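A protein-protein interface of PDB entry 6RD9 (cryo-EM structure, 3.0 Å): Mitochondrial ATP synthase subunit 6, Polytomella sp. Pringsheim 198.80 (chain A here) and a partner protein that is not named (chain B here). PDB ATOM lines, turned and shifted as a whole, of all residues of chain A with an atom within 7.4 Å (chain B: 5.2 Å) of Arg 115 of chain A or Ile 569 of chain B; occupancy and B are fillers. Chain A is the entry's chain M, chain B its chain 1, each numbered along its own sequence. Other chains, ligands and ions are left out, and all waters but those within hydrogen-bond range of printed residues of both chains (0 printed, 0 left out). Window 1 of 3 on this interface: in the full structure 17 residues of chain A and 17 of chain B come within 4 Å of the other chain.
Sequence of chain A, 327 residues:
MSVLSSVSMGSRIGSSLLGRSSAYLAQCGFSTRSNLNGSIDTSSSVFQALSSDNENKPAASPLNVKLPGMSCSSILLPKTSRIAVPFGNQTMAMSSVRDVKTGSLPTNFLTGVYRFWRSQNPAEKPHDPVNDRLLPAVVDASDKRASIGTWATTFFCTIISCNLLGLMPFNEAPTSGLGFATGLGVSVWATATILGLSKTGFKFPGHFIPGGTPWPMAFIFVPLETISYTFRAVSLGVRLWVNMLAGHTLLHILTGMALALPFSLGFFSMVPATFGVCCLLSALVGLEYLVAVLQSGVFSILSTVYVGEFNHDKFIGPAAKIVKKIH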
ATOM      1  N   PHE A 109      -0.634  10.049  28.661  1.00  0.00           N
ATOM      2  CA  PHE A 109       0.600  10.483  29.289  1.00  0.00           C
ATOM      3  C   PHE A 109       1.453  11.273  28.314  1.00  0.00           C
ATOM      4  O   PHE A 109       1.861  12.391  28.612  1.00  0.00           O
ATOM      5  CB  PHE A 109       1.356   9.281  29.822  1.00  0.00           C
ATOM      6  CG  PHE A 109       2.648   9.623  30.473  1.00  0.00           C
ATOM      7  CD1 PHE A 109       2.673  10.319  31.656  1.00  0.00           C
ATOM      8  CD2 PHE A 109       3.839   9.224  29.919  1.00  0.00           C
ATOM      9  CE1 PHE A 109       3.850  10.624  32.253  1.00  0.00           C
ATOM     10  CE2 PHE A 109       5.018   9.536  30.515  1.00  0.00           C
ATOM     11  CZ  PHE A 109       5.020  10.235  31.681  1.00  0.00           C
ATOM     12  N   LEU A 110       1.678  10.740  27.118  1.00  0.00           N
ATOM     13  CA  LEU A 110       2.469  11.445  26.123  1.00  0.00           C
ATOM     14  C   LEU A 110       1.801  12.688  25.575  1.00  0.00           C
ATOM     15  O   LEU A 110       2.492  13.523  25.007  1.00  0.00           O
ATOM     16  CB  LEU A 110       2.809  10.532  24.959  1.00  0.00           C
ATOM     17  CG  LEU A 110       4.238  10.022  24.882  1.00  0.00           C
ATOM     18  CD1 LEU A 110       5.148  11.211  24.800  1.00  0.00           C
ATOM     19  CD2 LEU A 110       4.605   9.171  26.051  1.00  0.00           C
ATOM     20  N   THR A 111       0.486  12.822  25.678  1.00  0.00           N
ATOM     21  CA  THR A 111      -0.146  14.090  25.343  1.00  0.00           C
ATOM     22  C   THR A 111       0.202  15.137  26.370  1.00  0.00           C
ATOM     23  O   THR A 111       0.549  16.262  26.028  1.00  0.00           O
ATOM     24  CB  THR A 111      -1.649  13.941  25.286  1.00  0.00           C
ATOM     25  OG1 THR A 111      -1.977  12.865  24.422  1.00  0.00           O
ATOM     26  CG2 THR A 111      -2.266  15.177  24.771  1.00  0.00           C
ATOM     27  N   GLY A 112       0.127  14.778  27.640  1.00  0.00           N
ATOM     28  CA  GLY A 112       0.454  15.724  28.675  1.00  0.00           C
ATOM     29  C   GLY A 112       1.925  16.024  28.757  1.00  0.00           C
ATOM     30  O   GLY A 112       2.306  17.112  29.169  1.00  0.00           O
ATOM     31  N   VAL A 113       2.768  15.075  28.374  1.00  0.00           N
ATOM     32  CA  VAL A 113       4.204  15.310  28.384  1.00  0.00           C
ATOM     33  C   VAL A 113       4.590  16.239  27.252  1.00  0.00           C
ATOM     34  O   VAL A 113       5.296  17.218  27.471  1.00  0.00           O
ATOM     35  CB  VAL A 113       4.965  13.981  28.321  1.00  0.00           C
ATOM     36  CG1 VAL A 113       6.392  14.212  28.030  1.00  0.00           C
ATOM     37  CG2 VAL A 113       4.854  13.277  29.602  1.00  0.00           C
ATOM     38  N   TYR A 114       4.092  15.984  26.042  1.00  0.00           N
ATOM     39  CA  TYR A 114       4.383  16.840  24.897  1.00  0.00           C
ATOM     40  C   TYR A 114       3.859  18.246  25.093  1.00  0.00           C
ATOM     41  O   TYR A 114       4.547  19.212  24.778  1.00  0.00           O
ATOM     42  CB  TYR A 114       3.774  16.267  23.622  1.00  0.00           C
ATOM     43  CG  TYR A 114       3.966  17.183  22.444  1.00  0.00           C
ATOM     44  CD1 TYR A 114       5.192  17.271  21.830  1.00  0.00           C
ATOM     45  CD2 TYR A 114       2.927  17.963  21.951  1.00  0.00           C
ATOM     46  CE1 TYR A 114       5.388  18.094  20.793  1.00  0.00           C
ATOM     47  CE2 TYR A 114       3.127  18.800  20.912  1.00  0.00           C
ATOM     48  CZ  TYR A 114       4.361  18.863  20.343  1.00  0.00           C
ATOM     49  OH  TYR A 114       4.575  19.691  19.285  1.00  0.00           O
ATOM     50  N   ARG A 115       2.640  18.381  25.596  1.00  0.00           N
ATOM     51  CA  ARG A 115       2.062  19.689  25.834  1.00  0.00           C
ATOM     52  C   ARG A 115       2.729  20.418  26.976  1.00  0.00           C
ATOM     53  O   ARG A 115       2.548  21.624  27.097  1.00  0.00           O
ATOM     54  CB  ARG A 115       0.588  19.561  26.147  1.00  0.00           C
ATOM     55  CG  ARG A 115      -0.242  19.252  24.976  1.00  0.00           C
ATOM     56  CD  ARG A 115      -1.640  18.935  25.391  1.00  0.00           C
ATOM     57  NE  ARG A 115      -2.255  20.032  26.101  1.00  0.00           N
ATOM     58  CZ  ARG A 115      -2.852  21.052  25.510  1.00  0.00           C
ATOM     59  NH1 ARG A 115      -3.389  22.011  26.230  1.00  0.00           N
ATOM     60  NH2 ARG A 115      -2.905  21.121  24.199  1.00  0.00           N
ATOM     61  N   PHE A 116       3.455  19.714  27.833  1.00  0.00           N
ATOM     62  CA  PHE A 116       4.253  20.375  28.849  1.00  0.00           C
ATOM     63  C   PHE A 116       5.486  21.014  28.244  1.00  0.00           C
ATOM     64  O   PHE A 116       5.756  22.188  28.477  1.00  0.00           O
ATOM     65  CB  PHE A 116       4.655  19.386  29.926  1.00  0.00           C
ATOM     66  CG  PHE A 116       5.417  20.000  31.043  1.00  0.00           C
ATOM     67  CD1 PHE A 116       4.774  20.736  32.002  1.00  0.00           C
ATOM     68  CD2 PHE A 116       6.770  19.837  31.146  1.00  0.00           C
ATOM     69  CE1 PHE A 116       5.473  21.301  33.019  1.00  0.00           C
ATOM     70  CE2 PHE A 116       7.461  20.400  32.161  1.00  0.00           C
ATOM     71  CZ  PHE A 116       6.817  21.126  33.093  1.00  0.00           C
ATOM     72  N   TRP A 117       6.249  20.259  27.462  1.00  0.00           N
ATOM     73  CA  TRP A 117       7.490  20.784  26.924  1.00  0.00           C
ATOM     74  C   TRP A 117       7.248  21.775  25.820  1.00  0.00           C
ATOM     75  O   TRP A 117       8.098  22.622  25.557  1.00  0.00           O
ATOM     76  CB  TRP A 117       8.367  19.660  26.418  1.00  0.00           C
ATOM     77  CG  TRP A 117       8.694  18.701  27.446  1.00  0.00           C
ATOM     78  CD1 TRP A 117       8.308  17.433  27.494  1.00  0.00           C
ATOM     79  CD2 TRP A 117       9.493  18.925  28.594  1.00  0.00           C
ATOM     80  NE1 TRP A 117       8.787  16.831  28.605  1.00  0.00           N
ATOM     81  CE2 TRP A 117       9.522  17.739  29.305  1.00  0.00           C
ATOM     82  CE3 TRP A 117      10.166  20.024  29.103  1.00  0.00           C
ATOM     83  CZ2 TRP A 117      10.201  17.608  30.477  1.00  0.00           C
ATOM     84  CZ3 TRP A 117      10.824  19.894  30.255  1.00  0.00           C
ATOM     85  CH2 TRP A 117      10.842  18.698  30.939  1.00  0.00           C
ATOM     86  N   ARG A 118       6.106  21.686  25.165  1.00  0.00           N
ATOM     87  CA  ARG A 118       5.724  22.715  24.220  1.00  0.00           C
ATOM     88  C   ARG A 118       5.370  24.009  24.938  1.00  0.00           C
ATOM     89  O   ARG A 118       5.602  25.091  24.408  1.00  0.00           O
ATOM     90  CB  ARG A 118       4.589  22.177  23.367  1.00  0.00           C
ATOM     91  CG  ARG A 118       3.948  23.098  22.400  1.00  0.00           C
ATOM     92  CD  ARG A 118       4.920  23.808  21.516  1.00  0.00           C
ATOM     93  NE  ARG A 118       4.282  24.845  20.721  1.00  0.00           N
ATOM     94  CZ  ARG A 118       3.919  26.035  21.173  1.00  0.00           C
ATOM     95  NH1 ARG A 118       4.101  26.374  22.426  1.00  0.00           N
ATOM     96  NH2 ARG A 118       3.353  26.896  20.363  1.00  0.00           N
ATOM     97  N   SER A 119       4.880  23.931  26.162  1.00  0.00           N
ATOM     98  CA  SER A 119       4.513  25.121  26.906  1.00  0.00           C
ATOM     99  C   SER A 119       5.703  25.884  27.437  1.00  0.00           C
ATOM    100  O   SER A 119       5.523  26.970  27.980  1.00  0.00           O
ATOM    101  CB  SER A 119       3.632  24.746  28.077  1.00  0.00           C
ATOM    102  OG  SER A 119       4.394  24.111  29.070  1.00  0.00           O
ATOM    103  N   GLN A 120       6.903  25.340  27.324  1.00  0.00           N
ATOM    104  CA  GLN A 120       8.061  25.990  27.904  1.00  0.00           C
ATOM    105  C   GLN A 120       8.571  27.110  27.033  1.00  0.00           C
ATOM    106  O   GLN A 120       9.143  28.070  27.545  1.00  0.00           O
ATOM    107  CB  GLN A 120       9.164  24.980  28.142  1.00  0.00           C
ATOM    108  CG  GLN A 120       8.801  23.844  29.038  1.00  0.00           C
ATOM    109  CD  GLN A 120       8.400  24.284  30.395  1.00  0.00           C
ATOM    110  OE1 GLN A 120       7.388  23.863  30.920  1.00  0.00           O
ATOM    111  NE2 GLN A 120       9.187  25.140  30.980  1.00  0.00           N
ATOM    112  N   PRO A 122       6.562  29.288  24.708  1.00  0.00           N
ATOM    113  CA  PRO A 122       5.311  29.647  24.060  1.00  0.00           C
ATOM    114  C   PRO A 122       5.518  30.668  22.962  1.00  0.00           C
ATOM    115  O   PRO A 122       6.493  31.413  22.949  1.00  0.00           O
ATOM    116  CB  PRO A 122       4.486  30.223  25.208  1.00  0.00           C
ATOM    117  CG  PRO A 122       5.447  30.722  26.126  1.00  0.00           C
ATOM    118  CD  PRO A 122       6.641  29.862  26.054  1.00  0.00           C
ATOM    119  N   ALA A 123       4.585  30.672  22.018  1.00  0.00           N
ATOM    120  CA  ALA A 123       4.597  31.654  20.953  1.00  0.00           C
ATOM    121  C   ALA A 123       4.210  33.011  21.505  1.00  0.00           C
ATOM    122  O   ALA A 123       3.488  33.118  22.494  1.00  0.00           O
ATOM    123  CB  ALA A 123       3.641  31.245  19.841  1.00  0.00           C
ATOM    124  N   GLY A 149       9.379  21.627  21.406  1.00  0.00           N
ATOM    125  CA  GLY A 149       8.375  20.802  22.028  1.00  0.00           C
ATOM    126  C   GLY A 149       8.572  19.341  21.742  1.00  0.00           C
ATOM    127  O   GLY A 149       8.310  18.513  22.600  1.00  0.00           O
ATOM    128  N   THR A 153      10.753  16.519  24.530  1.00  0.00           N
ATOM    129  CA  THR A 153      10.109  15.280  24.928  1.00  0.00           C
ATOM    130  C   THR A 153      10.770  14.077  24.306  1.00  0.00           C
ATOM    131  O   THR A 153      10.467  12.958  24.694  1.00  0.00           O
ATOM    132  CB  THR A 153       8.616  15.293  24.603  1.00  0.00           C
ATOM    133  OG1 THR A 153       8.035  14.049  24.972  1.00  0.00           O
ATOM    134  CG2 THR A 153       8.403  15.422  23.233  1.00  0.00           C
ATOM    135  N   ASP B 566       1.139  21.562  16.753  1.00  0.00           N
ATOM    136  CA  ASP B 566       0.794  22.340  17.922  1.00  0.00           C
ATOM    137  C   ASP B 566       0.076  23.624  17.555  1.00  0.00           C
ATOM    138  O   ASP B 566       0.222  24.619  18.252  1.00  0.00           O
ATOM    139  CB  ASP B 566       2.047  22.659  18.716  1.00  0.00           C
ATOM    140  CG  ASP B 566       3.072  23.388  17.902  1.00  0.00           C
ATOM    141  OD1 ASP B 566       3.207  23.098  16.705  1.00  0.00           O
ATOM    142  OD2 ASP B 566       3.758  24.257  18.459  1.00  0.00           O
ATOM    143  N   PHE B 567      -0.704  23.622  16.475  1.00  0.00           N
ATOM    144  CA  PHE B 567      -1.282  24.871  15.999  1.00  0.00           C
ATOM    145  C   PHE B 567      -2.361  25.384  16.923  1.00  0.00           C
ATOM    146  O   PHE B 567      -2.514  26.592  17.067  1.00  0.00           O
ATOM    147  CB  PHE B 567      -1.847  24.717  14.600  1.00  0.00           C
ATOM    148  CG  PHE B 567      -2.239  26.011  13.974  1.00  0.00           C
ATOM    149  CD1 PHE B 567      -1.313  27.016  13.814  1.00  0.00           C
ATOM    150  CD2 PHE B 567      -3.522  26.224  13.537  1.00  0.00           C
ATOM    151  CE1 PHE B 567      -1.664  28.210  13.241  1.00  0.00           C
ATOM    152  CE2 PHE B 567      -3.876  27.409  12.968  1.00  0.00           C
ATOM    153  CZ  PHE B 567      -2.947  28.400  12.815  1.00  0.00           C
ATOM    154  N   ASP B 568      -3.100  24.506  17.573  1.00  0.00           N
ATOM    155  CA  ASP B 568      -4.033  24.988  18.568  1.00  0.00           C
ATOM    156  C   ASP B 568      -3.352  25.400  19.861  1.00  0.00           C
ATOM    157  O   ASP B 568      -3.965  26.097  20.667  1.00  0.00           O
ATOM    158  CB  ASP B 568      -5.093  23.940  18.849  1.00  0.00           C
ATOM    159  CG  ASP B 568      -4.576  22.782  19.630  1.00  0.00           C
ATOM    160  OD1 ASP B 568      -3.681  22.074  19.149  1.00  0.00           O
ATOM    161  OD2 ASP B 568      -5.081  22.571  20.744  1.00  0.00           O
ATOM    162  N   ILE B 569      -2.118  24.965  20.098  1.00  0.00           N
ATOM    163  CA  ILE B 569      -1.370  25.493  21.226  1.00  0.00           C
ATOM    164  C   ILE B 569      -0.759  26.815  20.850  1.00  0.00           C
ATOM    165  O   ILE B 569      -0.575  27.676  21.703  1.00  0.00           O
ATOM    166  CB  ILE B 569      -0.295  24.503  21.696  1.00  0.00           C
ATOM    167  CG1 ILE B 569      -0.812  23.083  21.636  1.00  0.00           C
ATOM    168  CG2 ILE B 569       0.104  24.779  23.109  1.00  0.00           C
ATOM    169  CD1 ILE B 569       0.208  22.076  21.999  1.00  0.00           C
ATOM    170  N   THR B 570      -0.430  26.996  19.576  1.00  0.00           N
ATOM    171  CA  THR B 570       0.094  28.268  19.108  1.00  0.00           C
ATOM    172  C   THR B 570      -0.964  29.349  19.181  1.00  0.00           C
ATOM    173  O   THR B 570      -0.708  30.424  19.710  1.00  0.00           O
ATOM    174  CB  THR B 570       0.618  28.107  17.692  1.00  0.00           C
ATOM    175  OG1 THR B 570       1.819  27.343  17.723  1.00  0.00           O
ATOM    176  CG2 THR B 570       0.901  29.415  17.071  1.00  0.00           C
ATOM    177  N   LEU B 571      -2.177  29.059  18.724  1.00  0.00           N
ATOM    178  CA  LEU B 571      -3.281  29.998  18.840  1.00  0.00           C
ATOM    179  C   LEU B 571      -3.716  30.228  20.273  1.00  0.00           C
ATOM    180  O   LEU B 571      -4.350  31.239  20.547  1.00  0.00           O
ATOM    181  CB  LEU B 571      -4.479  29.513  18.046  1.00  0.00           C
ATOM    182  CG  LEU B 571      -4.283  29.424  16.552  1.00  0.00           C
ATOM    183  CD1 LEU B 571      -5.434  28.732  15.960  1.00  0.00           C
ATOM    184  CD2 LEU B 571      -4.145  30.779  15.972  1.00  0.00           C
ATOM    185  N   ASP B 572      -3.424  29.322  21.189  1.00  0.00           N
ATOM    186  CA  ASP B 572      -3.680  29.583  22.595  1.00  0.00           C
ATOM    187  C   ASP B 572      -2.575  30.373  23.254  1.00  0.00           C
ATOM    188  O   ASP B 572      -2.826  31.038  24.259  1.00  0.00           O
ATOM    189  CB  ASP B 572      -3.847  28.283  23.368  1.00  0.00           C
ATOM    190  CG  ASP B 572      -5.173  27.640  23.129  1.00  0.00           C
ATOM    191  OD1 ASP B 572      -5.908  28.131  22.260  1.00  0.00           O
ATOM    192  OD2 ASP B 572      -5.492  26.645  23.806  1.00  0.00           O
ATOM    193  N   ASP B 573      -1.353  30.281  22.739  1.00  0.00           N
ATOM    194  CA  ASP B 573      -0.271  31.101  23.256  1.00  0.00           C
ATOM    195  C   ASP B 573      -0.479  32.555  22.890  1.00  0.00           C
ATOM    196  O   ASP B 573      -0.284  33.443  23.721  1.00  0.00           O
ATOM    197  CB  ASP B 573       1.065  30.612  22.718  1.00  0.00           C
ATOM    198  CG  ASP B 573       1.489  29.312  23.323  1.00  0.00           C
ATOM    199  OD1 ASP B 573       0.927  28.926  24.358  1.00  0.00           O
ATOM    200  OD2 ASP B 573       2.390  28.664  22.768  1.00  0.00           O
ATOM    201  N   MET B 574      -0.891  32.822  21.662  1.00  0.00           N
ATOM    202  CA  MET B 574      -1.098  34.183  21.223  1.00  0.00           C
ATOM    203  C   MET B 574      -2.518  34.653  21.437  1.00  0.00           C
ATOM    204  O   MET B 574      -2.930  35.633  20.816  1.00  0.00           O
ATOM    205  CB  MET B 574      -0.689  34.340  19.764  1.00  0.00           C
ATOM    206  CG  MET B 574      -1.342  33.449  18.818  1.00  0.00           C
ATOM    207  SD  MET B 574      -0.531  33.511  17.235  1.00  0.00           S
ATOM    208  CE  MET B 574       1.170  33.463  17.717  1.00  0.00           C
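OD2 of Asp 566 of chain B lies within salt-bridge range of NH2 of Arg 118 of chain A, at 3.3 Å.
The guanidinium group (NH2) of Arg 118 of chain A lies within hydrogen-bond range of the side-chain hydroxyl (OG1) of Thr 570 of chain B (3.1 Å).
The side-chain carboxylate (OD2) of Asp 573 of chain B is in salt-bridge range of the guanidinium group (NH1) of Arg 118 of chain A, 2.9 Å away.
N of Ala 123 of chain A is in hydrogen-bond range of OD2 of Asp 573 of chain B (3.1 Å).
The backbone carbonyl oxygen (O) of Asp 566 of chain B is in hydrogen-bond range of the side-chain hydroxyl (OG1) of Thr 570 of chain B (3.2 Å).
Among the printed residues, merely in contact across the chains: Pro 122 of chain A with Asp 573 of chain B (3.3 Å), Arg 115 of chain A with Ile 569 of chain B (3.8 Å), Arg 118 of chain A with Ile 569 of chain B (3.9 Å), Tyr 114 of chain A with Asp 566 of chain B (3.9 Å) and Ala 123 of chain A with Met 574 of chain B (3.9 Å).
Of the printed residues of chain B, Arg 118 of chain A touches Asp 566 (2.4 Å), Ile 569 (3.9 Å), Thr 570 (3.1 Å) and Asp 573 (2.9 Å).
Of the printed residues of chain B, Pro 122 of chain A touches Asp 573 (3.3 Å).
Of the printed residues of chain A, Asp 566 of chain B touches Tyr 114 (3.9 Å) and Arg 118 (2.4 Å).
Of the printed residues of chain A, Thr 570 of chain B touches Arg 118 (3.1 Å).
Of the printed residues of chain A, Met 574 of chain B touches Ala 123 (3.9 Å).
The nearest residue of chain B that does not touch Arg 115 of chain A is Asp 568 of chain B (4.3 Å).
The nearest residue of chain A that does not touch Ile 569 of chain B is Tyr 114 of chain A (4.5 Å).
The nearest printed residue of chain A that does not touch Met 574 of chain B is Pro 122 of chain A (6.9 Å).
Of the 16 printed residues of chain A, 5 touch a printed residue of chain B.
Hydrophobic or aromatic side chains of chain A within 4 Å of the printed part of chain B: Tyr 114, Pro 122 and Ala 123.
Of the 9 printed residues of chain B, 5 touch a printed residue of chain A.
Printed residues of chain B that touch a printed residue of chain A: Asp 566, Ile 569, Thr 570, Asp 573 and Met 574.
Among the printed residues, 9 pairs touch across the chains.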
